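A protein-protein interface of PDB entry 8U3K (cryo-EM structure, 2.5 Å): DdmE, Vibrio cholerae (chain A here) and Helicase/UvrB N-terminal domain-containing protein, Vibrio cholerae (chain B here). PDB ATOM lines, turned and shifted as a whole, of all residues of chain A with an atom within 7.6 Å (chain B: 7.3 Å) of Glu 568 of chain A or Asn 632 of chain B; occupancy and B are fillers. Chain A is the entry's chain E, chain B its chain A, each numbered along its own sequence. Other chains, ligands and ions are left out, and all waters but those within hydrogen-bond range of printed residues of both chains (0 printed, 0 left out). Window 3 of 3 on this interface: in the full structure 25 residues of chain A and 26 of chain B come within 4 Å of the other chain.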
ATOM      1  N   LYS A 550      23.252  -9.359  18.360  1.00  0.00           N
ATOM      2  CA  LYS A 550      22.523  -8.199  17.866  1.00  0.00           C
ATOM      3  C   LYS A 550      21.430  -8.623  16.902  1.00  0.00           C
ATOM      4  O   LYS A 550      20.324  -8.072  16.922  1.00  0.00           O
ATOM      5  CB  LYS A 550      23.493  -7.234  17.192  1.00  0.00           C
ATOM      6  CG  LYS A 550      24.798  -7.082  17.945  1.00  0.00           C
ATOM      7  CD  LYS A 550      25.677  -6.023  17.321  1.00  0.00           C
ATOM      8  CE  LYS A 550      25.198  -4.634  17.689  1.00  0.00           C
ATOM      9  NZ  LYS A 550      25.530  -4.297  19.100  1.00  0.00           N
ATOM     10  N   LEU A 551      21.717  -9.617  16.063  1.00  0.00           N
ATOM     11  CA  LEU A 551      20.719 -10.108  15.122  1.00  0.00           C
ATOM     12  C   LEU A 551      19.536 -10.737  15.848  1.00  0.00           C
ATOM     13  O   LEU A 551      18.377 -10.518  15.476  1.00  0.00           O
ATOM     14  CB  LEU A 551      21.356 -11.108  14.162  1.00  0.00           C
ATOM     15  CG  LEU A 551      20.614 -11.243  12.837  1.00  0.00           C
ATOM     16  CD1 LEU A 551      20.264  -9.866  12.324  1.00  0.00           C
ATOM     17  CD2 LEU A 551      21.444 -12.003  11.831  1.00  0.00           C
ATOM     18  N   ILE A 554      17.437  -7.984  17.336  1.00  0.00           N
ATOM     19  CA  ILE A 554      16.652  -7.293  16.317  1.00  0.00           C
ATOM     20  C   ILE A 554      15.461  -8.142  15.895  1.00  0.00           C
ATOM     21  O   ILE A 554      14.340  -7.639  15.752  1.00  0.00           O
ATOM     22  CB  ILE A 554      17.542  -6.920  15.119  1.00  0.00           C
ATOM     23  CG1 ILE A 554      18.543  -5.841  15.521  1.00  0.00           C
ATOM     24  CG2 ILE A 554      16.702  -6.419  13.974  1.00  0.00           C
ATOM     25  CD1 ILE A 554      19.716  -5.724  14.583  1.00  0.00           C
ATOM     26  N   GLU A 557      12.825  -7.971  18.609  1.00  0.00           N
ATOM     27  CA  GLU A 557      12.070  -6.727  18.519  1.00  0.00           C
ATOM     28  C   GLU A 557      11.132  -6.729  17.321  1.00  0.00           C
ATOM     29  O   GLU A 557       9.982  -6.294  17.429  1.00  0.00           O
ATOM     30  CB  GLU A 557      13.026  -5.540  18.431  1.00  0.00           C
ATOM     31  CG  GLU A 557      13.852  -5.320  19.676  1.00  0.00           C
ATOM     32  CD  GLU A 557      14.765  -4.125  19.549  1.00  0.00           C
ATOM     33  OE1 GLU A 557      14.273  -3.042  19.179  1.00  0.00           O
ATOM     34  OE2 GLU A 557      15.973  -4.263  19.826  1.00  0.00           O
ATOM     35  N   TRP A 558      11.600  -7.232  16.186  1.00  0.00           N
ATOM     36  CA  TRP A 558      10.836  -7.184  14.956  1.00  0.00           C
ATOM     37  C   TRP A 558       9.643  -8.137  15.022  1.00  0.00           C
ATOM     38  O   TRP A 558       9.559  -9.027  15.872  1.00  0.00           O
ATOM     39  CB  TRP A 558      11.732  -7.527  13.764  1.00  0.00           C
ATOM     40  CG  TRP A 558      11.075  -7.320  12.450  1.00  0.00           C
ATOM     41  CD1 TRP A 558      10.685  -8.280  11.570  1.00  0.00           C
ATOM     42  CD2 TRP A 558      10.705  -6.071  11.874  1.00  0.00           C
ATOM     43  NE1 TRP A 558      10.097  -7.706  10.475  1.00  0.00           N
ATOM     44  CE2 TRP A 558      10.098  -6.347  10.638  1.00  0.00           C
ATOM     45  CE3 TRP A 558      10.833  -4.743  12.282  1.00  0.00           C
ATOM     46  CZ2 TRP A 558       9.620  -5.346   9.807  1.00  0.00           C
ATOM     47  CZ3 TRP A 558      10.358  -3.754  11.459  1.00  0.00           C
ATOM     48  CH2 TRP A 558       9.755  -4.057  10.237  1.00  0.00           C
ATOM     49  N   PRO A 563       9.434  -9.143   6.469  1.00  0.00           N
ATOM     50  CA  PRO A 563      10.882  -9.112   6.259  1.00  0.00           C
ATOM     51  C   PRO A 563      11.500  -7.864   6.867  1.00  0.00           C
ATOM     52  O   PRO A 563      10.865  -6.812   6.960  1.00  0.00           O
ATOM     53  CB  PRO A 563      11.018  -9.120   4.734  1.00  0.00           C
ATOM     54  CG  PRO A 563       9.761  -9.745   4.256  1.00  0.00           C
ATOM     55  CD  PRO A 563       8.703  -9.259   5.199  1.00  0.00           C
ATOM     56  N   LEU A 564      12.744  -7.996   7.294  1.00  0.00           N
ATOM     57  CA  LEU A 564      13.411  -6.925   8.012  1.00  0.00           C
ATOM     58  C   LEU A 564      13.893  -5.863   7.032  1.00  0.00           C
ATOM     59  O   LEU A 564      14.598  -6.195   6.074  1.00  0.00           O
ATOM     60  CB  LEU A 564      14.577  -7.485   8.804  1.00  0.00           C
ATOM     61  CG  LEU A 564      15.140  -6.617   9.919  1.00  0.00           C
ATOM     62  CD1 LEU A 564      14.147  -6.525  11.048  1.00  0.00           C
ATOM     63  CD2 LEU A 564      16.440  -7.205  10.409  1.00  0.00           C
ATOM     64  N   PRO A 565      13.516  -4.600   7.208  1.00  0.00           N
ATOM     65  CA  PRO A 565      14.060  -3.545   6.350  1.00  0.00           C
ATOM     66  C   PRO A 565      15.519  -3.288   6.678  1.00  0.00           C
ATOM     67  O   PRO A 565      15.988  -3.577   7.780  1.00  0.00           O
ATOM     68  CB  PRO A 565      13.191  -2.328   6.685  1.00  0.00           C
ATOM     69  CG  PRO A 565      11.983  -2.883   7.350  1.00  0.00           C
ATOM     70  CD  PRO A 565      12.458  -4.089   8.086  1.00  0.00           C
ATOM     71  N   PHE A 566      16.236  -2.725   5.704  1.00  0.00           N
ATOM     72  CA  PHE A 566      17.660  -2.472   5.888  1.00  0.00           C
ATOM     73  C   PHE A 566      17.907  -1.455   6.991  1.00  0.00           C
ATOM     74  O   PHE A 566      18.975  -1.444   7.612  1.00  0.00           O
ATOM     75  CB  PHE A 566      18.283  -1.995   4.578  1.00  0.00           C
ATOM     76  CG  PHE A 566      19.642  -1.392   4.748  1.00  0.00           C
ATOM     77  CD1 PHE A 566      20.722  -2.180   5.081  1.00  0.00           C
ATOM     78  CD2 PHE A 566      19.831  -0.034   4.611  1.00  0.00           C
ATOM     79  CE1 PHE A 566      21.967  -1.626   5.255  1.00  0.00           C
ATOM     80  CE2 PHE A 566      21.073   0.521   4.784  1.00  0.00           C
ATOM     81  CZ  PHE A 566      22.141  -0.276   5.106  1.00  0.00           C
ATOM     82  N   ASP A 567      16.920  -0.601   7.267  1.00  0.00           N
ATOM     83  CA  ASP A 567      17.112   0.460   8.248  1.00  0.00           C
ATOM     84  C   ASP A 567      17.320  -0.093   9.652  1.00  0.00           C
ATOM     85  O   ASP A 567      17.881   0.595  10.511  1.00  0.00           O
ATOM     86  CB  ASP A 567      15.922   1.411   8.215  1.00  0.00           C
ATOM     87  CG  ASP A 567      15.517   1.780   6.803  1.00  0.00           C
ATOM     88  OD1 ASP A 567      14.779   0.997   6.171  1.00  0.00           O
ATOM     89  OD2 ASP A 567      15.948   2.847   6.319  1.00  0.00           O
ATOM     90  N   GLU A 568      16.878  -1.326   9.907  1.00  0.00           N
ATOM     91  CA  GLU A 568      17.151  -1.964  11.187  1.00  0.00           C
ATOM     92  C   GLU A 568      18.601  -2.409  11.313  1.00  0.00           C
ATOM     93  O   GLU A 568      19.118  -2.486  12.432  1.00  0.00           O
ATOM     94  CB  GLU A 568      16.228  -3.161  11.380  1.00  0.00           C
ATOM     95  CG  GLU A 568      14.789  -2.884  11.004  1.00  0.00           C
ATOM     96  CD  GLU A 568      14.209  -1.707  11.756  1.00  0.00           C
ATOM     97  OE1 GLU A 568      14.376  -1.651  12.991  1.00  0.00           O
ATOM     98  OE2 GLU A 568      13.583  -0.838  11.113  1.00  0.00           O
ATOM     99  N   PHE A 569      19.273  -2.688  10.197  1.00  0.00           N
ATOM    100  CA  PHE A 569      20.651  -3.153  10.224  1.00  0.00           C
ATOM    101  C   PHE A 569      21.646  -2.067  10.590  1.00  0.00           C
ATOM    102  O   PHE A 569      22.830  -2.377  10.752  1.00  0.00           O
ATOM    103  CB  PHE A 569      21.063  -3.716   8.869  1.00  0.00           C
ATOM    104  CG  PHE A 569      20.393  -4.994   8.508  1.00  0.00           C
ATOM    105  CD1 PHE A 569      19.141  -4.997   7.940  1.00  0.00           C
ATOM    106  CD2 PHE A 569      21.028  -6.195   8.717  1.00  0.00           C
ATOM    107  CE1 PHE A 569      18.534  -6.168   7.594  1.00  0.00           C
ATOM    108  CE2 PHE A 569      20.422  -7.370   8.376  1.00  0.00           C
ATOM    109  CZ  PHE A 569      19.173  -7.357   7.812  1.00  0.00           C
ATOM    110  N   SER A 570      21.204  -0.815  10.712  1.00  0.00           N
ATOM    111  CA  SER A 570      22.136   0.300  10.845  1.00  0.00           C
ATOM    112  C   SER A 570      22.994   0.192  12.098  1.00  0.00           C
ATOM    113  O   SER A 570      24.058   0.813  12.173  1.00  0.00           O
ATOM    114  CB  SER A 570      21.366   1.619  10.841  1.00  0.00           C
ATOM    115  OG  SER A 570      20.525   1.706   9.704  1.00  0.00           O
ATOM    116  N   THR A 571      22.558  -0.586  13.086  1.00  0.00           N
ATOM    117  CA  THR A 571      23.390  -0.796  14.263  1.00  0.00           C
ATOM    118  C   THR A 571      24.601  -1.667  13.953  1.00  0.00           C
ATOM    119  O   THR A 571      25.636  -1.542  14.616  1.00  0.00           O
ATOM    120  CB  THR A 571      22.562  -1.414  15.389  1.00  0.00           C
ATOM    121  OG1 THR A 571      23.423  -1.770  16.478  1.00  0.00           O
ATOM    122  CG2 THR A 571      21.820  -2.647  14.898  1.00  0.00           C
ATOM    123  N   ILE A 572      24.502  -2.540  12.957  1.00  0.00           N
ATOM    124  CA  ILE A 572      25.587  -3.450  12.612  1.00  0.00           C
ATOM    125  C   ILE A 572      26.449  -2.771  11.557  1.00  0.00           C
ATOM    126  O   ILE A 572      26.034  -2.617  10.407  1.00  0.00           O
ATOM    127  CB  ILE A 572      25.055  -4.795  12.109  1.00  0.00           C
ATOM    128  CG1 ILE A 572      24.036  -5.361  13.089  1.00  0.00           C
ATOM    129  CG2 ILE A 572      26.187  -5.772  11.939  1.00  0.00           C
ATOM    130  CD1 ILE A 572      23.364  -6.612  12.592  1.00  0.00           C
ATOM    131  N   TYR A 583      27.880  -9.500   6.164  1.00  0.00           N
ATOM    132  CA  TYR A 583      27.357  -8.740   5.036  1.00  0.00           C
ATOM    133  C   TYR A 583      27.735  -9.381   3.710  1.00  0.00           C
ATOM    134  O   TYR A 583      26.955  -9.343   2.754  1.00  0.00           O
ATOM    135  CB  TYR A 583      27.845  -7.303   5.102  1.00  0.00           C
ATOM    136  CG  TYR A 583      27.001  -6.438   5.992  1.00  0.00           C
ATOM    137  CD1 TYR A 583      25.671  -6.207   5.702  1.00  0.00           C
ATOM    138  CD2 TYR A 583      27.534  -5.852   7.120  1.00  0.00           C
ATOM    139  CE1 TYR A 583      24.900  -5.420   6.509  1.00  0.00           C
ATOM    140  CE2 TYR A 583      26.769  -5.062   7.930  1.00  0.00           C
ATOM    141  CZ  TYR A 583      25.455  -4.847   7.620  1.00  0.00           C
ATOM    142  OH  TYR A 583      24.692  -4.056   8.438  1.00  0.00           O
ATOM    143  N   LYS A 594      25.825  -3.392   2.391  1.00  0.00           N
ATOM    144  CA  LYS A 594      26.895  -2.516   2.834  1.00  0.00           C
ATOM    145  C   LYS A 594      28.187  -2.903   2.141  1.00  0.00           C
ATOM    146  O   LYS A 594      28.396  -4.057   1.767  1.00  0.00           O
ATOM    147  CB  LYS A 594      27.085  -2.574   4.349  1.00  0.00           C
ATOM    148  CG  LYS A 594      26.173  -1.663   5.127  1.00  0.00           C
ATOM    149  CD  LYS A 594      26.637  -1.553   6.560  1.00  0.00           C
ATOM    150  CE  LYS A 594      25.941  -0.428   7.290  1.00  0.00           C
ATOM    151  NZ  LYS A 594      24.581  -0.825   7.727  1.00  0.00           N
ATOM    152  N   LYS B 629       3.900  -1.119  17.678  1.00  0.00           N
ATOM    153  CA  LYS B 629       5.090  -1.136  16.847  1.00  0.00           C
ATOM    154  C   LYS B 629       5.867   0.140  17.083  1.00  0.00           C
ATOM    155  O   LYS B 629       5.276   1.195  17.310  1.00  0.00           O
ATOM    156  CB  LYS B 629       4.744  -1.235  15.379  1.00  0.00           C
ATOM    157  CG  LYS B 629       4.406  -2.618  14.918  1.00  0.00           C
ATOM    158  CD  LYS B 629       5.611  -3.269  14.282  1.00  0.00           C
ATOM    159  CE  LYS B 629       6.215  -2.384  13.212  1.00  0.00           C
ATOM    160  NZ  LYS B 629       7.666  -2.646  13.061  1.00  0.00           N
ATOM    161  N   TYR B 630       7.183   0.045  17.036  1.00  0.00           N
ATOM    162  CA  TYR B 630       8.040   1.214  17.113  1.00  0.00           C
ATOM    163  C   TYR B 630       8.715   1.382  15.765  1.00  0.00           C
ATOM    164  O   TYR B 630       9.437   0.492  15.312  1.00  0.00           O
ATOM    165  CB  TYR B 630       9.054   1.082  18.246  1.00  0.00           C
ATOM    166  CG  TYR B 630       8.443   1.338  19.599  1.00  0.00           C
ATOM    167  CD1 TYR B 630       8.408   2.606  20.131  1.00  0.00           C
ATOM    168  CD2 TYR B 630       7.888   0.313  20.333  1.00  0.00           C
ATOM    169  CE1 TYR B 630       7.838   2.843  21.349  1.00  0.00           C
ATOM    170  CE2 TYR B 630       7.320   0.546  21.550  1.00  0.00           C
ATOM    171  CZ  TYR B 630       7.299   1.812  22.052  1.00  0.00           C
ATOM    172  OH  TYR B 630       6.726   2.054  23.269  1.00  0.00           O
ATOM    173  N   LEU B 631       8.466   2.511  15.123  1.00  0.00           N
ATOM    174  CA  LEU B 631       8.881   2.752  13.752  1.00  0.00           C
ATOM    175  C   LEU B 631      10.052   3.716  13.754  1.00  0.00           C
ATOM    176  O   LEU B 631       9.975   4.779  14.374  1.00  0.00           O
ATOM    177  CB  LEU B 631       7.728   3.336  12.942  1.00  0.00           C
ATOM    178  CG  LEU B 631       6.440   2.537  12.934  1.00  0.00           C
ATOM    179  CD1 LEU B 631       5.294   3.453  12.672  1.00  0.00           C
ATOM    180  CD2 LEU B 631       6.519   1.501  11.865  1.00  0.00           C
ATOM    181  N   ASN B 632      11.128   3.349  13.070  1.00  0.00           N
ATOM    182  CA  ASN B 632      12.198   4.287  12.784  1.00  0.00           C
ATOM    183  C   ASN B 632      12.112   4.739  11.332  1.00  0.00           C
ATOM    184  O   ASN B 632      11.119   4.507  10.644  1.00  0.00           O
ATOM    185  CB  ASN B 632      13.554   3.674  13.112  1.00  0.00           C
ATOM    186  CG  ASN B 632      13.505   2.184  13.181  1.00  0.00           C
ATOM    187  OD1 ASN B 632      12.607   1.558  12.627  1.00  0.00           O
ATOM    188  ND2 ASN B 632      14.467   1.594  13.872  1.00  0.00           N
ATOM    189  N   SER B 633      13.153   5.420  10.867  1.00  0.00           N
ATOM    190  CA  SER B 633      13.173   5.915   9.504  1.00  0.00           C
ATOM    191  C   SER B 633      13.200   4.760   8.511  1.00  0.00           C
ATOM    192  O   SER B 633      13.659   3.658   8.806  1.00  0.00           O
ATOM    193  CB  SER B 633      14.376   6.819   9.284  1.00  0.00           C
ATOM    194  OG  SER B 633      14.645   7.570  10.447  1.00  0.00           O
ATOM    195  N   ARG B 634      12.678   5.027   7.318  1.00  0.00           N
ATOM    196  CA  ARG B 634      12.463   4.018   6.296  1.00  0.00           C
ATOM    197  C   ARG B 634      12.946   4.557   4.951  1.00  0.00           C
ATOM    198  O   ARG B 634      12.204   4.596   3.979  1.00  0.00           O
ATOM    199  CB  ARG B 634      10.994   3.619   6.236  1.00  0.00           C
ATOM    200  CG  ARG B 634      10.516   2.846   7.436  1.00  0.00           C
ATOM    201  CD  ARG B 634      10.984   1.411   7.381  1.00  0.00           C
ATOM    202  NE  ARG B 634      10.912   0.761   8.684  1.00  0.00           N
ATOM    203  CZ  ARG B 634       9.787   0.390   9.284  1.00  0.00           C
ATOM    204  NH1 ARG B 634       9.835  -0.190  10.473  1.00  0.00           N
ATOM    205  NH2 ARG B 634       8.615   0.586   8.699  1.00  0.00           N
ATOM    206  N   ASP B 635      14.204   5.008   4.924  1.00  0.00           N
ATOM    207  CA  ASP B 635      14.714   5.844   3.837  1.00  0.00           C
ATOM    208  C   ASP B 635      14.503   5.225   2.462  1.00  0.00           C
ATOM    209  O   ASP B 635      14.107   5.923   1.524  1.00  0.00           O
ATOM    210  CB  ASP B 635      16.195   6.123   4.061  1.00  0.00           C
ATOM    211  CG  ASP B 635      16.427   7.200   5.090  1.00  0.00           C
ATOM    212  OD1 ASP B 635      17.584   7.378   5.517  1.00  0.00           O
ATOM    213  OD2 ASP B 635      15.446   7.869   5.475  1.00  0.00           O
ATOM    214  N   ARG B 671      12.646  13.650   6.171  1.00  0.00           N
ATOM    215  CA  ARG B 671      12.772  12.241   5.823  1.00  0.00           C
ATOM    216  C   ARG B 671      12.586  11.356   7.041  1.00  0.00           C
ATOM    217  O   ARG B 671      12.084  10.237   6.931  1.00  0.00           O
ATOM    218  CB  ARG B 671      14.135  11.974   5.195  1.00  0.00           C
ATOM    219  CG  ARG B 671      14.266  12.484   3.791  1.00  0.00           C
ATOM    220  CD  ARG B 671      15.675  12.329   3.271  1.00  0.00           C
ATOM    221  NE  ARG B 671      15.966  10.942   2.955  1.00  0.00           N
ATOM    222  CZ  ARG B 671      15.639  10.361   1.809  1.00  0.00           C
ATOM    223  NH1 ARG B 671      15.937   9.089   1.601  1.00  0.00           N
ATOM    224  NH2 ARG B 671      15.015  11.052   0.869  1.00  0.00           N
ATOM    225  N   SER B 672      12.976  11.844   8.214  1.00  0.00           N
ATOM    226  CA  SER B 672      12.754  11.062   9.421  1.00  0.00           C
ATOM    227  C   SER B 672      11.277  11.026   9.787  1.00  0.00           C
ATOM    228  O   SER B 672      10.697   9.950   9.946  1.00  0.00           O
ATOM    229  CB  SER B 672      13.574  11.625  10.573  1.00  0.00           C
ATOM    230  OG  SER B 672      12.811  12.572  11.289  1.00  0.00           O
ATOM    231  N   SER B 675       8.815   9.359   6.916  1.00  0.00           N
ATOM    232  CA  SER B 675       8.900   7.922   6.698  1.00  0.00           C
ATOM    233  C   SER B 675       8.112   7.157   7.747  1.00  0.00           C
ATOM    234  O   SER B 675       7.414   6.190   7.432  1.00  0.00           O
ATOM    235  CB  SER B 675      10.357   7.489   6.718  1.00  0.00           C
ATOM    236  OG  SER B 675      11.094   8.206   5.760  1.00  0.00           O
ATOM    237  N   LYS B 676       8.219   7.573   9.007  1.00  0.00           N
ATOM    238  CA  LYS B 676       7.492   6.907  10.077  1.00  0.00           C
ATOM    239  C   LYS B 676       5.988   7.070   9.913  1.00  0.00           C
ATOM    240  O   LYS B 676       5.226   6.111  10.090  1.00  0.00           O
ATOM    241  CB  LYS B 676       7.947   7.463  11.417  1.00  0.00           C
ATOM    242  CG  LYS B 676       9.431   7.383  11.608  1.00  0.00           C
ATOM    243  CD  LYS B 676       9.842   7.984  12.919  1.00  0.00           C
ATOM    244  CE  LYS B 676      11.300   8.355  12.893  1.00  0.00           C
ATOM    245  NZ  LYS B 676      11.816   8.595  14.253  1.00  0.00           N
ATOM    246  N   LEU B 677       5.545   8.277   9.569  1.00  0.00           N
ATOM    247  CA  LEU B 677       4.127   8.529   9.361  1.00  0.00           C
ATOM    248  C   LEU B 677       3.582   7.681   8.226  1.00  0.00           C
ATOM    249  O   LEU B 677       2.509   7.081   8.338  1.00  0.00           O
ATOM    250  CB  LEU B 677       3.913  10.007   9.065  1.00  0.00           C
ATOM    251  CG  LEU B 677       2.505  10.424   8.685  1.00  0.00           C
ATOM    252  CD1 LEU B 677       1.575  10.211   9.839  1.00  0.00           C
ATOM    253  CD2 LEU B 677       2.497  11.859   8.261  1.00  0.00           C
ATOM    254  N   ALA B 679       4.871   4.879   6.950  1.00  0.00           N
ATOM    255  CA  ALA B 679       4.910   3.466   7.300  1.00  0.00           C
ATOM    256  C   ALA B 679       3.739   3.088   8.193  1.00  0.00           C
ATOM    257  O   ALA B 679       3.116   2.035   8.002  1.00  0.00           O
ATOM    258  CB  ALA B 679       6.232   3.135   7.975  1.00  0.00           C
ATOM    259  N   VAL B 900       4.273   3.920  17.015  1.00  0.00           N
ATOM    260  CA  VAL B 900       4.978   4.848  17.881  1.00  0.00           C
ATOM    261  C   VAL B 900       6.284   5.239  17.224  1.00  0.00           C
ATOM    262  O   VAL B 900       6.977   4.390  16.660  1.00  0.00           O
ATOM    263  CB  VAL B 900       5.246   4.248  19.270  1.00  0.00           C
ATOM    264  CG1 VAL B 900       5.498   5.337  20.250  1.00  0.00           C
ATOM    265  CG2 VAL B 900       4.078   3.444  19.722  1.00  0.00           C
ATOM    266  N   ASP B 901       6.605   6.521  17.285  1.00  0.00           N
ATOM    267  CA  ASP B 901       7.927   6.990  16.919  1.00  0.00           C
ATOM    268  C   ASP B 901       8.968   6.263  17.757  1.00  0.00           C
ATOM    269  O   ASP B 901       8.794   6.086  18.962  1.00  0.00           O
ATOM    270  CB  ASP B 901       7.992   8.495  17.153  1.00  0.00           C
ATOM    271  CG  ASP B 901       9.203   9.134  16.547  1.00  0.00           C
ATOM    272  OD1 ASP B 901      10.104   8.414  16.096  1.00  0.00           O
ATOM    273  OD2 ASP B 901       9.258  10.375  16.525  1.00  0.00           O
ATOM    274  N   SER B 902      10.047   5.816  17.115  1.00  0.00           N
ATOM    275  CA  SER B 902      11.064   5.070  17.843  1.00  0.00           C
ATOM    276  C   SER B 902      11.881   5.955  18.761  1.00  0.00           C
ATOM    277  O   SER B 902      12.567   5.441  19.647  1.00  0.00           O
ATOM    278  CB  SER B 902      11.994   4.354  16.879  1.00  0.00           C
ATOM    279  OG  SER B 902      12.789   5.285  16.183  1.00  0.00           O
ATOM    280  N   GLY B 903      11.839   7.271  18.569  1.00  0.00           N
ATOM    281  CA  GLY B 903      12.448   8.167  19.527  1.00  0.00           C
ATOM    282  C   GLY B 903      11.748   8.168  20.864  1.00  0.00           C
ATOM    283  O   GLY B 903      12.304   8.657  21.848  1.00  0.00           O
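Printed residues of chain A that touch a printed residue of chain B: Trp 558, Asp 567 and Glu 568. Hydrophobic or aromatic side chains of chain A that line the printed part of chain B: Trp 558. Among the printed residues, Asp or Glu carboxylates within 4 Å of a Lys or Arg side-chain nitrogen of the other chain: Glu 568 of chain A with Arg 634 of chain B (3.9 Å).
CZ3 of Trp 558 of chain A touches NZ of Lys 629 of chain B, 3.3 Å away. Arg 634 of chain B touches Trp 558 of chain A. Asp 567 of chain A touches Arg 634 of chain B.
O of Lys 629 of chain B lies within hydrogen-bond range of N of Val 900 of chain B, at 2.9 Å. O of Asp 567 of chain A sits at hydrogen-bond distance from OG of Ser 570 of chain A (3.0 Å).
Glu 568 of chain A touches just these residues of chain B: Asn 632 and Arg 634. Of the printed residues of chain B, Asp 567 of chain A touches Ser 633, Arg 634 and Asp 635. Of the printed residues of chain A, Arg 634 of chain B touches Trp 558 (3.7 Å), Asp 567 (3.7 Å) and Glu 568 (3.9 Å). Printed residues of chain A within 4 Å of Ser 633 of chain B: Asp 567 (3.2 Å). The nearest residue of chain A that does not touch Asn 632 of chain B is Asp 567 of chain A (4.9 Å). The nearest printed residue of chain B that does not touch Asp 567 of chain A is Asn 632 of chain B (4.9 Å).
The side-chain carboxylate of Glu 568 of chain A sits close to the side-chain amide oxygen of Asn 632 of chain B (3.0 Å). The side-chain carboxylate (OE2) of Glu 568 of chain A is in salt-bridge range of the guanidinium group (NH1) of Arg 634 of chain B (3.9 Å). The side-chain carboxylate (OD2) of Asp 567 of chain A sits at hydrogen-bond distance from the backbone NH (N) of Asp 635 of chain B (3.1 Å). The backbone carbonyl oxygen (O) of Ser 633 of chain B lies close to the side-chain carboxylate (OD2) of Asp 567 of chain A.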
